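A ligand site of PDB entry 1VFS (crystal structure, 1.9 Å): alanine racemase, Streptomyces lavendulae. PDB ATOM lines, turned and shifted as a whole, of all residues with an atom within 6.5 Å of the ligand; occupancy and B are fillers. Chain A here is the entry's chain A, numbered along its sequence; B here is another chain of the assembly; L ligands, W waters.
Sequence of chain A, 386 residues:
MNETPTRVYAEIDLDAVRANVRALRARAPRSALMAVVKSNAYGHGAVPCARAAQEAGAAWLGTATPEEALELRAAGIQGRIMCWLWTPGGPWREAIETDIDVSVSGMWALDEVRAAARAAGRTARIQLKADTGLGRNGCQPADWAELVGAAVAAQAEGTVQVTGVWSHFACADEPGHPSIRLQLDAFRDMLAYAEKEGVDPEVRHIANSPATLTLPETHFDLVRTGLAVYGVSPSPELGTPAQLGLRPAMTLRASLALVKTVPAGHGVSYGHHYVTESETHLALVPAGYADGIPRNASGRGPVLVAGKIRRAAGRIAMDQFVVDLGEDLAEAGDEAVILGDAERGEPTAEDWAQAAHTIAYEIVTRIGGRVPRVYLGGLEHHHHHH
N of Leu 227 is in hydrogen-bond range of O4 of the ligand (3.0 Å). A nitrogen (N1) of the ligand is in hydrogen-bond range of the guanidinium group of Arg 224 (3.0 Å). The guanidinium group (NH1) of Arg 136 sits at hydrogen-bond distance from an oxygen (O1) of the ligand (2.8 Å). The side-chain hydroxyl (OH) of Tyr 42 sits at hydrogen-bond distance from an oxygen (O4) of the ligand, at 2.7 Å. N of Ser 209 sits close to O3 of the ligand (2.9 Å). OH of Tyr 289 of chain B is in hydrogen-bond range of O7 of the ligand, at 3.2 Å. The side-chain amino group (NZ) of Lys 38 lies close to a nitrogen (N2) of the ligand (2.8 Å). The side-chain hydroxyl (OH) of Tyr 361 sits at hydrogen-bond distance from an oxygen (O5) of the ligand, 2.6 Å away. OG of Ser 209 is in hydrogen-bond range of O3 of the ligand, 2.5 Å away. O3 of the ligand is in hydrogen-bond range of N of Gly 226 (2.8 Å). An oxygen (O6) of the ligand is in hydrogen-bond range of the side-chain hydroxyl of Tyr 270 of chain B (2.7 Å).
NH2 of Arg 224 is in hydrogen-bond range of ND1 of His 168. N of Tyr 289 of chain B lies within hydrogen-bond range of O of Met 318 of chain B, at 3.2 Å. The side-chain amino group of Lys 38 is in salt-bridge range of the side-chain carboxylate of Asp 319 of chain B, at 3.4 Å. The guanidinium group (NH2) of Arg 224 lies within hydrogen-bond range of the backbone carbonyl oxygen (O) of Ser 167 (3.1 Å). NH1 of Arg 136 lies within salt-bridge range of OQ2 of KCX 129 (2.6 Å). The side-chain hydroxyl (OH) of Tyr 42 is in hydrogen-bond range of the side-chain amino group (NZ) of Lys 38, 3.4 Å away. The backbone carbonyl oxygen of Thr 225 lies within hydrogen-bond range of the backbone NH of Val 36, 3.0 Å away. The guanidinium group of Arg 136 sits at hydrogen-bond distance from the side-chain amide oxygen of Gln 320 of chain B (3.3 Å).
Water W1 lies within hydrogen-bond range of N3 of the ligand (2.9 Å) and OH of Tyr 289 of chain B (3.3 Å). Water W3 lies within hydrogen-bond range of the indole nitrogen of Trp 84, the side-chain carboxylate of Asp 319 of chain B and an oxygen (O1) of the ligand. Water W4 lies within hydrogen-bond range of O5 of the ligand (3.1 Å), ND2 of Asn 208 (3.4 Å) and OH of Tyr 270 of chain B (3.5 Å).
The backbone NH of Met 318 of chain B lies close to a nitrogen (N3) of the ligand. Merely in contact with the ligand: Val 36 (3.9 Å), Trp 84 (3.7 Å), KCX 129 (3.999 Å), Trp 166 (3.8 Å), His 168 (3.5 Å), Asn 208 (3.6 Å), Pro 210 (3.7 Å), Thr 225 (3.7 Å) and Ala 317 of chain B (3.3 Å). Hydrophobic or aromatic side chains within 4 Å of the ligand: Val 36, Tyr 42, Trp 84, Trp 166, His 168, Pro 210, Leu 227, Tyr 361, Tyr 270 of chain B, Ala 317 of chain B and Met 318 of chain B. 20 residues have an atom within 4 Å of the ligand: Val 36, Lys 38, Tyr 42, Trp 84, KCX 129, Arg 136, Trp 166, His 168, Asn 208, Ser 209, Pro 210, Arg 224, Thr 225, Gly 226, Leu 227, Tyr 361, Tyr 270 of chain B, Tyr 289 of chain B, Ala 317 of chain B and Met 318 of chain B. The nearest printed residue that does not touch the ligand is Asp 319 of chain B (4.3 Å).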
ATOM      1  N   MET A  34      13.436   1.450 -26.649  1.00  0.00           N
ATOM      2  CA  MET A  34      13.408   0.045 -27.026  1.00  0.00           C
ATOM      3  C   MET A  34      12.622  -0.093 -28.333  1.00  0.00           C
ATOM      4  O   MET A  34      11.432   0.238 -28.391  1.00  0.00           O
ATOM      5  CB  MET A  34      12.725  -0.818 -25.963  1.00  0.00           C
ATOM      6  CG  MET A  34      12.356  -2.208 -26.504  1.00  0.00           C
ATOM      7  SD  MET A  34      11.553  -3.324 -25.351  1.00  0.00           S
ATOM      8  CE  MET A  34      12.561  -3.060 -23.888  1.00  0.00           C
ATOM      9  N   VAL A  36      10.640  -2.176 -30.775  1.00  0.00           N
ATOM     10  CA  VAL A  36       9.914  -3.434 -30.747  1.00  0.00           C
ATOM     11  C   VAL A  36       9.854  -3.964 -32.178  1.00  0.00           C
ATOM     12  O   VAL A  36       9.213  -3.371 -33.054  1.00  0.00           O
ATOM     13  CB  VAL A  36       8.504  -3.251 -30.180  1.00  0.00           C
ATOM     14  CG1 VAL A  36       7.871  -4.609 -29.958  1.00  0.00           C
ATOM     15  CG2 VAL A  36       8.569  -2.463 -28.875  1.00  0.00           C
ATOM     16  N   LYS A  38       8.964  -7.291 -32.933  1.00  0.00           N
ATOM     17  CA  LYS A  38       8.259  -8.562 -32.939  1.00  0.00           C
ATOM     18  C   LYS A  38       7.402  -8.678 -34.202  1.00  0.00           C
ATOM     19  O   LYS A  38       7.175  -7.691 -34.894  1.00  0.00           O
ATOM     20  CB  LYS A  38       7.376  -8.704 -31.699  1.00  0.00           C
ATOM     21  CG  LYS A  38       6.183  -7.743 -31.615  1.00  0.00           C
ATOM     22  CD  LYS A  38       5.892  -7.390 -30.155  1.00  0.00           C
ATOM     23  CE  LYS A  38       4.410  -7.298 -29.842  1.00  0.00           C
ATOM     24  NZ  LYS A  38       3.676  -6.406 -30.755  1.00  0.00           N
ATOM     25  N   TYR A  42       6.728  -6.026 -37.465  1.00  0.00           N
ATOM     26  CA  TYR A  42       5.426  -5.579 -37.919  1.00  0.00           C
ATOM     27  C   TYR A  42       5.333  -5.721 -39.437  1.00  0.00           C
ATOM     28  O   TYR A  42       4.811  -4.840 -40.128  1.00  0.00           O
ATOM     29  CB  TYR A  42       5.185  -4.122 -37.509  1.00  0.00           C
ATOM     30  CG  TYR A  42       4.933  -3.921 -36.034  1.00  0.00           C
ATOM     31  CD1 TYR A  42       5.658  -4.639 -35.072  1.00  0.00           C
ATOM     32  CD2 TYR A  42       3.977  -2.999 -35.587  1.00  0.00           C
ATOM     33  CE1 TYR A  42       5.441  -4.438 -33.707  1.00  0.00           C
ATOM     34  CE2 TYR A  42       3.762  -2.797 -34.213  1.00  0.00           C
ATOM     35  CZ  TYR A  42       4.493  -3.513 -33.283  1.00  0.00           C
ATOM     36  OH  TYR A  42       4.296  -3.310 -31.933  1.00  0.00           O
ATOM     37  N   TRP A  84       8.838 -11.178 -23.775  1.00  0.00           N
ATOM     38  CA  TRP A  84       7.898 -11.343 -22.675  1.00  0.00           C
ATOM     39  C   TRP A  84       6.821 -12.413 -22.771  1.00  0.00           C
ATOM     40  O   TRP A  84       6.177 -12.718 -21.774  1.00  0.00           O
ATOM     41  CB  TRP A  84       7.221  -9.997 -22.427  1.00  0.00           C
ATOM     42  CG  TRP A  84       6.768  -9.303 -23.702  1.00  0.00           C
ATOM     43  CD1 TRP A  84       5.612  -9.546 -24.397  1.00  0.00           C
ATOM     44  CD2 TRP A  84       7.443  -8.247 -24.401  1.00  0.00           C
ATOM     45  NE1 TRP A  84       5.530  -8.701 -25.478  1.00  0.00           N
ATOM     46  CE2 TRP A  84       6.632  -7.888 -25.508  1.00  0.00           C
ATOM     47  CE3 TRP A  84       8.646  -7.563 -24.196  1.00  0.00           C
ATOM     48  CZ2 TRP A  84       7.001  -6.879 -26.403  1.00  0.00           C
ATOM     49  CZ3 TRP A  84       9.006  -6.549 -25.089  1.00  0.00           C
ATOM     50  CH2 TRP A  84       8.187  -6.218 -26.183  1.00  0.00           C
ATOM     51  N   KCX A 129       6.597  -8.135 -14.494  1.00  0.00           N
ATOM     52  CA  KCX A 129       5.493  -7.422 -15.116  1.00  0.00           C
ATOM     53  CB  KCX A 129       5.041  -8.116 -16.407  1.00  0.00           C
ATOM     54  CG  KCX A 129       4.290  -7.163 -17.311  1.00  0.00           C
ATOM     55  CD  KCX A 129       3.202  -7.846 -18.095  1.00  0.00           C
ATOM     56  CE  KCX A 129       2.328  -6.794 -18.756  1.00  0.00           C
ATOM     57  NZ  KCX A 129       2.295  -6.972 -20.222  1.00  0.00           N
ATOM     58  C   KCX A 129       4.284  -7.309 -14.187  1.00  0.00           C
ATOM     59  O   KCX A 129       3.857  -8.303 -13.588  1.00  0.00           O
ATOM     60  CX  KCX A 129       1.102  -7.308 -20.972  1.00  0.00           C
ATOM     61  OQ1 KCX A 129       0.006  -7.467 -20.382  1.00  0.00           O
ATOM     62  OQ2 KCX A 129       1.177  -7.487 -22.205  1.00  0.00           O
ATOM     63  N   ARG A 136      -4.369  -8.473 -19.247  1.00  0.00           N
ATOM     64  CA  ARG A 136      -3.731  -9.390 -20.189  1.00  0.00           C
ATOM     65  C   ARG A 136      -2.702 -10.213 -19.428  1.00  0.00           C
ATOM     66  O   ARG A 136      -3.060 -11.147 -18.706  1.00  0.00           O
ATOM     67  CB  ARG A 136      -3.048  -8.588 -21.299  1.00  0.00           C
ATOM     68  CG  ARG A 136      -2.650  -9.407 -22.517  1.00  0.00           C
ATOM     69  CD  ARG A 136      -2.439  -8.509 -23.727  1.00  0.00           C
ATOM     70  NE  ARG A 136      -1.090  -7.952 -23.759  1.00  0.00           N
ATOM     71  CZ  ARG A 136      -0.658  -7.100 -24.675  1.00  0.00           C
ATOM     72  NH1 ARG A 136       0.580  -6.638 -24.623  1.00  0.00           N
ATOM     73  NH2 ARG A 136      -1.471  -6.697 -25.652  1.00  0.00           N
ATOM     74  N   TRP A 166       7.731  -3.324 -15.057  1.00  0.00           N
ATOM     75  CA  TRP A 166       6.998  -2.639 -16.107  1.00  0.00           C
ATOM     76  C   TRP A 166       5.545  -3.054 -16.239  1.00  0.00           C
ATOM     77  O   TRP A 166       5.077  -3.966 -15.567  1.00  0.00           O
ATOM     78  CB  TRP A 166       7.692  -2.895 -17.437  1.00  0.00           C
ATOM     79  CG  TRP A 166       7.695  -4.364 -17.805  1.00  0.00           C
ATOM     80  CD1 TRP A 166       8.227  -5.395 -17.083  1.00  0.00           C
ATOM     81  CD2 TRP A 166       7.101  -4.951 -18.971  1.00  0.00           C
ATOM     82  NE1 TRP A 166       8.017  -6.592 -17.726  1.00  0.00           N
ATOM     83  CE2 TRP A 166       7.325  -6.351 -18.880  1.00  0.00           C
ATOM     84  CE3 TRP A 166       6.407  -4.441 -20.076  1.00  0.00           C
ATOM     85  CZ2 TRP A 166       6.871  -7.242 -19.866  1.00  0.00           C
ATOM     86  CZ3 TRP A 166       5.967  -5.326 -21.055  1.00  0.00           C
ATOM     87  CH2 TRP A 166       6.199  -6.715 -20.946  1.00  0.00           C
ATOM     88  N   SER A 167       4.847  -2.370 -17.153  1.00  0.00           N
ATOM     89  CA  SER A 167       3.455  -2.643 -17.455  1.00  0.00           C
ATOM     90  C   SER A 167       3.121  -2.227 -18.896  1.00  0.00           C
ATOM     91  O   SER A 167       4.006  -1.835 -19.665  1.00  0.00           O
ATOM     92  CB  SER A 167       2.530  -1.905 -16.485  1.00  0.00           C
ATOM     93  OG  SER A 167       1.283  -2.565 -16.385  1.00  0.00           O
ATOM     94  N   HIS A 168       1.833  -2.300 -19.258  1.00  0.00           N
ATOM     95  CA  HIS A 168       1.366  -1.959 -20.603  1.00  0.00           C
ATOM     96  C   HIS A 168      -0.044  -1.355 -20.554  1.00  0.00           C
ATOM     97  O   HIS A 168      -0.946  -1.907 -19.942  1.00  0.00           O
ATOM     98  CB  HIS A 168       1.380  -3.233 -21.462  1.00  0.00           C
ATOM     99  CG  HIS A 168       1.234  -2.990 -22.930  1.00  0.00           C
ATOM    100  ND1 HIS A 168       1.987  -2.046 -23.615  1.00  0.00           N
ATOM    101  CD2 HIS A 168       0.394  -3.541 -23.851  1.00  0.00           C
ATOM    102  CE1 HIS A 168       1.620  -2.033 -24.881  1.00  0.00           C
ATOM    103  NE2 HIS A 168       0.667  -2.925 -25.051  1.00  0.00           N
ATOM    104  N   ALA A 207       5.389   2.946 -21.143  1.00  0.00           N
ATOM    105  CA  ALA A 207       4.994   3.649 -22.359  1.00  0.00           C
ATOM    106  C   ALA A 207       5.169   2.896 -23.688  1.00  0.00           C
ATOM    107  O   ALA A 207       6.199   2.291 -23.952  1.00  0.00           O
ATOM    108  CB  ALA A 207       5.742   4.978 -22.429  1.00  0.00           C
ATOM    109  N   ASN A 208       4.124   2.935 -24.523  1.00  0.00           N
ATOM    110  CA  ASN A 208       4.169   2.318 -25.846  1.00  0.00           C
ATOM    111  C   ASN A 208       4.199   3.497 -26.815  1.00  0.00           C
ATOM    112  O   ASN A 208       4.402   4.631 -26.370  1.00  0.00           O
ATOM    113  CB  ASN A 208       2.957   1.414 -26.091  1.00  0.00           C
ATOM    114  CG  ASN A 208       1.639   2.111 -25.865  1.00  0.00           C
ATOM    115  OD1 ASN A 208       1.589   3.297 -25.545  1.00  0.00           O
ATOM    116  ND2 ASN A 208       0.540   1.372 -26.037  1.00  0.00           N
ATOM    117  N   SER A 209       4.008   3.256 -28.108  1.00  0.00           N
ATOM    118  CA  SER A 209       4.048   4.354 -29.084  1.00  0.00           C
ATOM    119  C   SER A 209       3.091   5.509 -28.800  1.00  0.00           C
ATOM    120  O   SER A 209       3.511   6.663 -28.774  1.00  0.00           O
ATOM    121  CB  SER A 209       3.806   3.830 -30.506  1.00  0.00           C
ATOM    122  OG  SER A 209       4.976   3.226 -31.026  1.00  0.00           O
ATOM    123  N   PRO A 210       1.787   5.232 -28.607  1.00  0.00           N
ATOM    124  CA  PRO A 210       0.873   6.358 -28.331  1.00  0.00           C
ATOM    125  C   PRO A 210       1.178   7.089 -27.022  1.00  0.00           C
ATOM    126  O   PRO A 210       1.151   8.318 -26.977  1.00  0.00           O
ATOM    127  CB  PRO A 210      -0.511   5.709 -28.345  1.00  0.00           C
ATOM    128  CG  PRO A 210      -0.257   4.251 -28.081  1.00  0.00           C
ATOM    129  CD  PRO A 210       1.080   3.944 -28.652  1.00  0.00           C
ATOM    130  N   ARG A 224       8.933   1.755 -24.878  1.00  0.00           N
ATOM    131  CA  ARG A 224       8.870   0.695 -25.863  1.00  0.00           C
ATOM    132  C   ARG A 224       8.021   1.107 -27.059  1.00  0.00           C
ATOM    133  O   ARG A 224       6.786   1.086 -26.995  1.00  0.00           O
ATOM    134  CB  ARG A 224       8.279  -0.555 -25.228  1.00  0.00           C
ATOM    135  CG  ARG A 224       8.908  -0.941 -23.914  1.00  0.00           C
ATOM    136  CD  ARG A 224       8.369  -2.268 -23.427  1.00  0.00           C
ATOM    137  NE  ARG A 224       6.901  -2.305 -23.466  1.00  0.00           N
ATOM    138  CZ  ARG A 224       6.120  -1.720 -22.566  1.00  0.00           C
ATOM    139  NH1 ARG A 224       6.661  -1.062 -21.549  1.00  0.00           N
ATOM    140  NH2 ARG A 224       4.802  -1.785 -22.686  1.00  0.00           N
ATOM    141  N   THR A 225       8.685   1.499 -28.140  1.00  0.00           N
ATOM    142  CA  THR A 225       7.987   1.939 -29.350  1.00  0.00           C
ATOM    143  C   THR A 225       8.015   0.881 -30.437  1.00  0.00           C
ATOM    144  O   THR A 225       9.077   0.336 -30.785  1.00  0.00           O
ATOM    145  CB  THR A 225       8.603   3.246 -29.914  1.00  0.00           C
ATOM    146  OG1 THR A 225      10.026   3.103 -30.015  1.00  0.00           O
ATOM    147  CG2 THR A 225       8.286   4.426 -29.001  1.00  0.00           C
ATOM    148  N   GLY A 226       6.843   0.583 -30.979  1.00  0.00           N
ATOM    149  CA  GLY A 226       6.731  -0.405 -32.031  1.00  0.00           C
ATOM    150  C   GLY A 226       6.280   0.228 -33.342  1.00  0.00           C
ATOM    151  O   GLY A 226       7.104   0.564 -34.196  1.00  0.00           O
ATOM    152  N   LEU A 227       4.969   0.407 -33.484  1.00  0.00           N
ATOM    153  CA  LEU A 227       4.384   0.965 -34.699  1.00  0.00           C
ATOM    154  C   LEU A 227       4.988   2.259 -35.238  1.00  0.00           C
ATOM    155  O   LEU A 227       5.278   2.350 -36.438  1.00  0.00           O
ATOM    156  CB  LEU A 227       2.877   1.171 -34.534  1.00  0.00           C
ATOM    157  CG  LEU A 227       2.134   1.314 -35.874  1.00  0.00           C
ATOM    158  CD1 LEU A 227       2.094  -0.031 -36.572  1.00  0.00           C
ATOM    159  CD2 LEU A 227       0.727   1.825 -35.664  1.00  0.00           C
ATOM    160  N   ALA A 228       5.157   3.250 -34.363  1.00  0.00           N
ATOM    161  CA  ALA A 228       5.693   4.560 -34.766  1.00  0.00           C
ATOM    162  C   ALA A 228       7.082   4.484 -35.388  1.00  0.00           C
ATOM    163  O   ALA A 228       7.456   5.348 -36.169  1.00  0.00           O
ATOM    164  CB  ALA A 228       5.706   5.511 -33.576  1.00  0.00           C
ATOM    165  N   PRO A 234      -0.489   5.403 -34.402  1.00  0.00           N
ATOM    166  CA  PRO A 234      -1.291   4.460 -33.635  1.00  0.00           C
ATOM    167  C   PRO A 234      -2.801   4.676 -33.809  1.00  0.00           C
ATOM    168  O   PRO A 234      -3.593   3.781 -33.571  1.00  0.00           O
ATOM    169  CB  PRO A 234      -0.838   4.683 -32.181  1.00  0.00           C
ATOM    170  CG  PRO A 234       0.474   5.395 -32.279  1.00  0.00           C
ATOM    171  CD  PRO A 234       0.418   6.199 -33.547  1.00  0.00           C
ATOM    172  N   ILE A 359      -7.591  -1.758 -37.613  1.00  0.00           N
ATOM    173  CA  ILE A 359      -6.593  -0.748 -37.279  1.00  0.00           C
ATOM    174  C   ILE A 359      -5.335  -0.948 -38.099  1.00  0.00           C
ATOM    175  O   ILE A 359      -5.035  -2.063 -38.531  1.00  0.00           O
ATOM    176  CB  ILE A 359      -6.231  -0.804 -35.761  1.00  0.00           C
ATOM    177  CG1 ILE A 359      -5.825  -2.220 -35.358  1.00  0.00           C
ATOM    178  CG2 ILE A 359      -7.417  -0.349 -34.937  1.00  0.00           C
ATOM    179  CD1 ILE A 359      -5.286  -2.307 -33.948  1.00  0.00           C
ATOM    180  N   TYR A 361      -2.372  -1.176 -37.314  1.00  0.00           N
ATOM    181  CA  TYR A 361      -1.472  -2.162 -36.717  1.00  0.00           C
ATOM    182  C   TYR A 361      -1.581  -3.515 -37.420  1.00  0.00           C
ATOM    183  O   TYR A 361      -0.569  -4.151 -37.718  1.00  0.00           O
ATOM    184  CB  TYR A 361      -1.823  -2.390 -35.245  1.00  0.00           C
ATOM    185  CG  TYR A 361      -1.295  -1.374 -34.255  1.00  0.00           C
ATOM    186  CD1 TYR A 361      -0.074  -1.574 -33.599  1.00  0.00           C
ATOM    187  CD2 TYR A 361      -2.034  -0.249 -33.914  1.00  0.00           C
ATOM    188  CE1 TYR A 361       0.382  -0.674 -32.625  1.00  0.00           C
ATOM    189  CE2 TYR A 361      -1.593   0.644 -32.946  1.00  0.00           C
ATOM    190  CZ  TYR A 361      -0.383   0.424 -32.306  1.00  0.00           C
ATOM    191  OH  TYR A 361       0.036   1.316 -31.334  1.00  0.00           O
ATOM    192  N   TYR B 270      -7.280  -4.098 -24.944  1.00  0.00           N
ATOM    193  CA  TYR B 270      -7.332  -2.757 -25.520  1.00  0.00           C
ATOM    194  C   TYR B 270      -8.741  -2.183 -25.582  1.00  0.00           C
ATOM    195  O   TYR B 270      -9.710  -2.895 -25.886  1.00  0.00           O
ATOM    196  CB  TYR B 270      -6.726  -2.766 -26.923  1.00  0.00           C
ATOM    197  CG  TYR B 270      -5.254  -3.127 -26.934  1.00  0.00           C
ATOM    198  CD1 TYR B 270      -4.370  -2.550 -26.015  1.00  0.00           C
ATOM    199  CD2 TYR B 270      -4.751  -4.064 -27.846  1.00  0.00           C
ATOM    200  CE1 TYR B 270      -3.028  -2.891 -25.999  1.00  0.00           C
ATOM    201  CE2 TYR B 270      -3.403  -4.418 -27.831  1.00  0.00           C
ATOM    202  CZ  TYR B 270      -2.555  -3.826 -26.905  1.00  0.00           C
ATOM    203  OH  TYR B 270      -1.230  -4.190 -26.873  1.00  0.00           O
ATOM    204  N   TYR B 289      -3.438 -11.807 -33.877  1.00  0.00           N
ATOM    205  CA  TYR B 289      -3.655 -11.595 -35.306  1.00  0.00           C
ATOM    206  C   TYR B 289      -2.386 -11.675 -36.159  1.00  0.00           C
ATOM    207  O   TYR B 289      -2.474 -11.856 -37.377  1.00  0.00           O
ATOM    208  CB  TYR B 289      -4.448 -10.295 -35.594  1.00  0.00           C
ATOM    209  CG  TYR B 289      -3.858  -8.970 -35.137  1.00  0.00           C
ATOM    210  CD1 TYR B 289      -2.720  -8.430 -35.747  1.00  0.00           C
ATOM    211  CD2 TYR B 289      -4.492  -8.230 -34.138  1.00  0.00           C
ATOM    212  CE1 TYR B 289      -2.217  -7.181 -35.357  1.00  0.00           C
ATOM    213  CE2 TYR B 289      -3.998  -6.977 -33.747  1.00  0.00           C
ATOM    214  CZ  TYR B 289      -2.858  -6.459 -34.356  1.00  0.00           C
ATOM    215  OH  TYR B 289      -2.391  -5.218 -33.967  1.00  0.00           O
ATOM    216  N   ILE B 316      -8.813  -8.827 -29.589  1.00  0.00           N
ATOM    217  CA  ILE B 316      -7.769  -9.804 -29.845  1.00  0.00           C
ATOM    218  C   ILE B 316      -6.532  -8.969 -30.215  1.00  0.00           C
ATOM    219  O   ILE B 316      -6.623  -8.083 -31.071  1.00  0.00           O
ATOM    220  CB  ILE B 316      -8.148 -10.722 -31.019  1.00  0.00           C
ATOM    221  CG1 ILE B 316      -9.242 -11.697 -30.576  1.00  0.00           C
ATOM    222  CG2 ILE B 316      -6.918 -11.486 -31.518  1.00  0.00           C
ATOM    223  CD1 ILE B 316      -9.778 -12.599 -31.687  1.00  0.00           C
ATOM    224  N   ALA B 317      -5.404  -9.232 -29.564  1.00  0.00           N
ATOM    225  CA  ALA B 317      -4.178  -8.471 -29.822  1.00  0.00           C
ATOM    226  C   ALA B 317      -3.252  -9.131 -30.839  1.00  0.00           C
ATOM    227  O   ALA B 317      -3.524 -10.225 -31.334  1.00  0.00           O
ATOM    228  CB  ALA B 317      -3.420  -8.245 -28.507  1.00  0.00           C
ATOM    229  N   MET B 318      -2.143  -8.452 -31.137  1.00  0.00           N
ATOM    230  CA  MET B 318      -1.166  -8.951 -32.117  1.00  0.00           C
ATOM    231  C   MET B 318      -0.600 -10.327 -31.825  1.00  0.00           C
ATOM    232  O   MET B 318      -0.479 -11.161 -32.724  1.00  0.00           O
ATOM    233  CB  MET B 318       0.002  -7.962 -32.239  1.00  0.00           C
ATOM    234  CG  MET B 318       0.831  -8.161 -33.500  1.00  0.00           C
ATOM    235  SD  MET B 318       2.201  -6.990 -33.763  1.00  0.00           S
ATOM    236  CE  MET B 318       1.377  -5.593 -34.443  1.00  0.00           C
ATOM    237  N   ASP B 319      -0.254 -10.581 -30.554  1.00  0.00           N
ATOM    238  CA  ASP B 319       0.337 -11.854 -30.173  1.00  0.00           C
ATOM    239  C   ASP B 319      -0.442 -12.704 -29.182  1.00  0.00           C
ATOM    240  O   ASP B 319      -0.040 -13.835 -28.895  1.00  0.00           O
ATOM    241  CB  ASP B 319       1.760 -11.625 -29.607  1.00  0.00           C
ATOM    242  CG  ASP B 319       2.455 -10.407 -30.200  1.00  0.00           C
ATOM    243  OD1 ASP B 319       3.094 -10.535 -31.272  1.00  0.00           O
ATOM    244  OD2 ASP B 319       2.382  -9.325 -29.589  1.00  0.00           O
ATOM    245  N   GLN B 320      -1.547 -12.187 -28.648  1.00  0.00           N
ATOM    246  CA  GLN B 320      -2.305 -12.958 -27.658  1.00  0.00           C
ATOM    247  C   GLN B 320      -3.707 -12.414 -27.432  1.00  0.00           C
ATOM    248  O   GLN B 320      -4.049 -11.325 -27.902  1.00  0.00           O
ATOM    249  CB  GLN B 320      -1.553 -12.944 -26.323  1.00  0.00           C
ATOM    250  CG  GLN B 320      -1.572 -11.577 -25.635  1.00  0.00           C
ATOM    251  CD  GLN B 320      -0.236 -11.209 -25.011  1.00  0.00           C
ATOM    252  OE1 GLN B 320       0.442 -10.285 -25.462  1.00  0.00           O
ATOM    253  NE2 GLN B 320       0.142 -11.910 -23.955  1.00  0.00           N
HETATM  254  N1  LIG L   1       5.132  -3.606 -25.467  1.00  0.00           N
HETATM  255  C1  LIG L   1       4.160  -4.608 -25.438  1.00  0.00           C
HETATM  256  C2  LIG L   1       4.008  -5.556 -24.266  1.00  0.00           C
HETATM  257  C3  LIG L   1       3.314  -4.697 -26.520  1.00  0.00           C
HETATM  258  O1  LIG L   1       2.366  -5.642 -26.542  1.00  0.00           O
HETATM  259  C4  LIG L   1       3.461  -3.775 -27.596  1.00  0.00           C
HETATM  260  C5  LIG L   1       2.464  -3.713 -28.699  1.00  0.00           C
HETATM  261  C6  LIG L   1       4.498  -2.791 -27.524  1.00  0.00           C
HETATM  262  C7  LIG L   1       5.295  -2.731 -26.470  1.00  0.00           C
HETATM  263  C8  LIG L   1       4.747  -1.786 -28.650  1.00  0.00           C
HETATM  264  O2  LIG L   1       3.620  -0.903 -28.758  1.00  0.00           O
HETATM  265  P1  LIG L   1       3.303   0.012 -30.020  1.00  0.00           P
HETATM  266  O3  LIG L   1       4.310   1.060 -30.019  1.00  0.00           O
HETATM  267  O4  LIG L   1       3.367  -0.829 -31.215  1.00  0.00           O
HETATM  268  O5  LIG L   1       1.954   0.533 -29.813  1.00  0.00           O
HETATM  269  N2  LIG L   1       1.932  -5.052 -29.106  1.00  0.00           N
HETATM  270  C9  LIG L   1       0.805  -5.065 -29.919  1.00  0.00           C
HETATM  271  C10 LIG L   1      -0.468  -5.593 -29.536  1.00  0.00           C
HETATM  272  O6  LIG L   1      -0.702  -6.322 -28.407  1.00  0.00           O
HETATM  273  N3  LIG L   1      -1.365  -5.227 -30.410  1.00  0.00           N
HETATM  274  O7  LIG L   1      -0.734  -4.458 -31.372  1.00  0.00           O
HETATM  275  C11 LIG L   1       0.574  -4.361 -31.079  1.00  0.00           C
HETATM  276  O   HOH W   1      -3.929  -4.162 -31.240  1.00  0.00           O
HETATM  277  O   HOH W   2       0.019  -8.817 -28.186  1.00  0.00           O
HETATM  278  O   HOH W   3       3.220  -8.397 -27.057  1.00  0.00           O
HETATM  279  O   HOH W   4       0.045  -1.232 -28.110  1.00  0.00           O
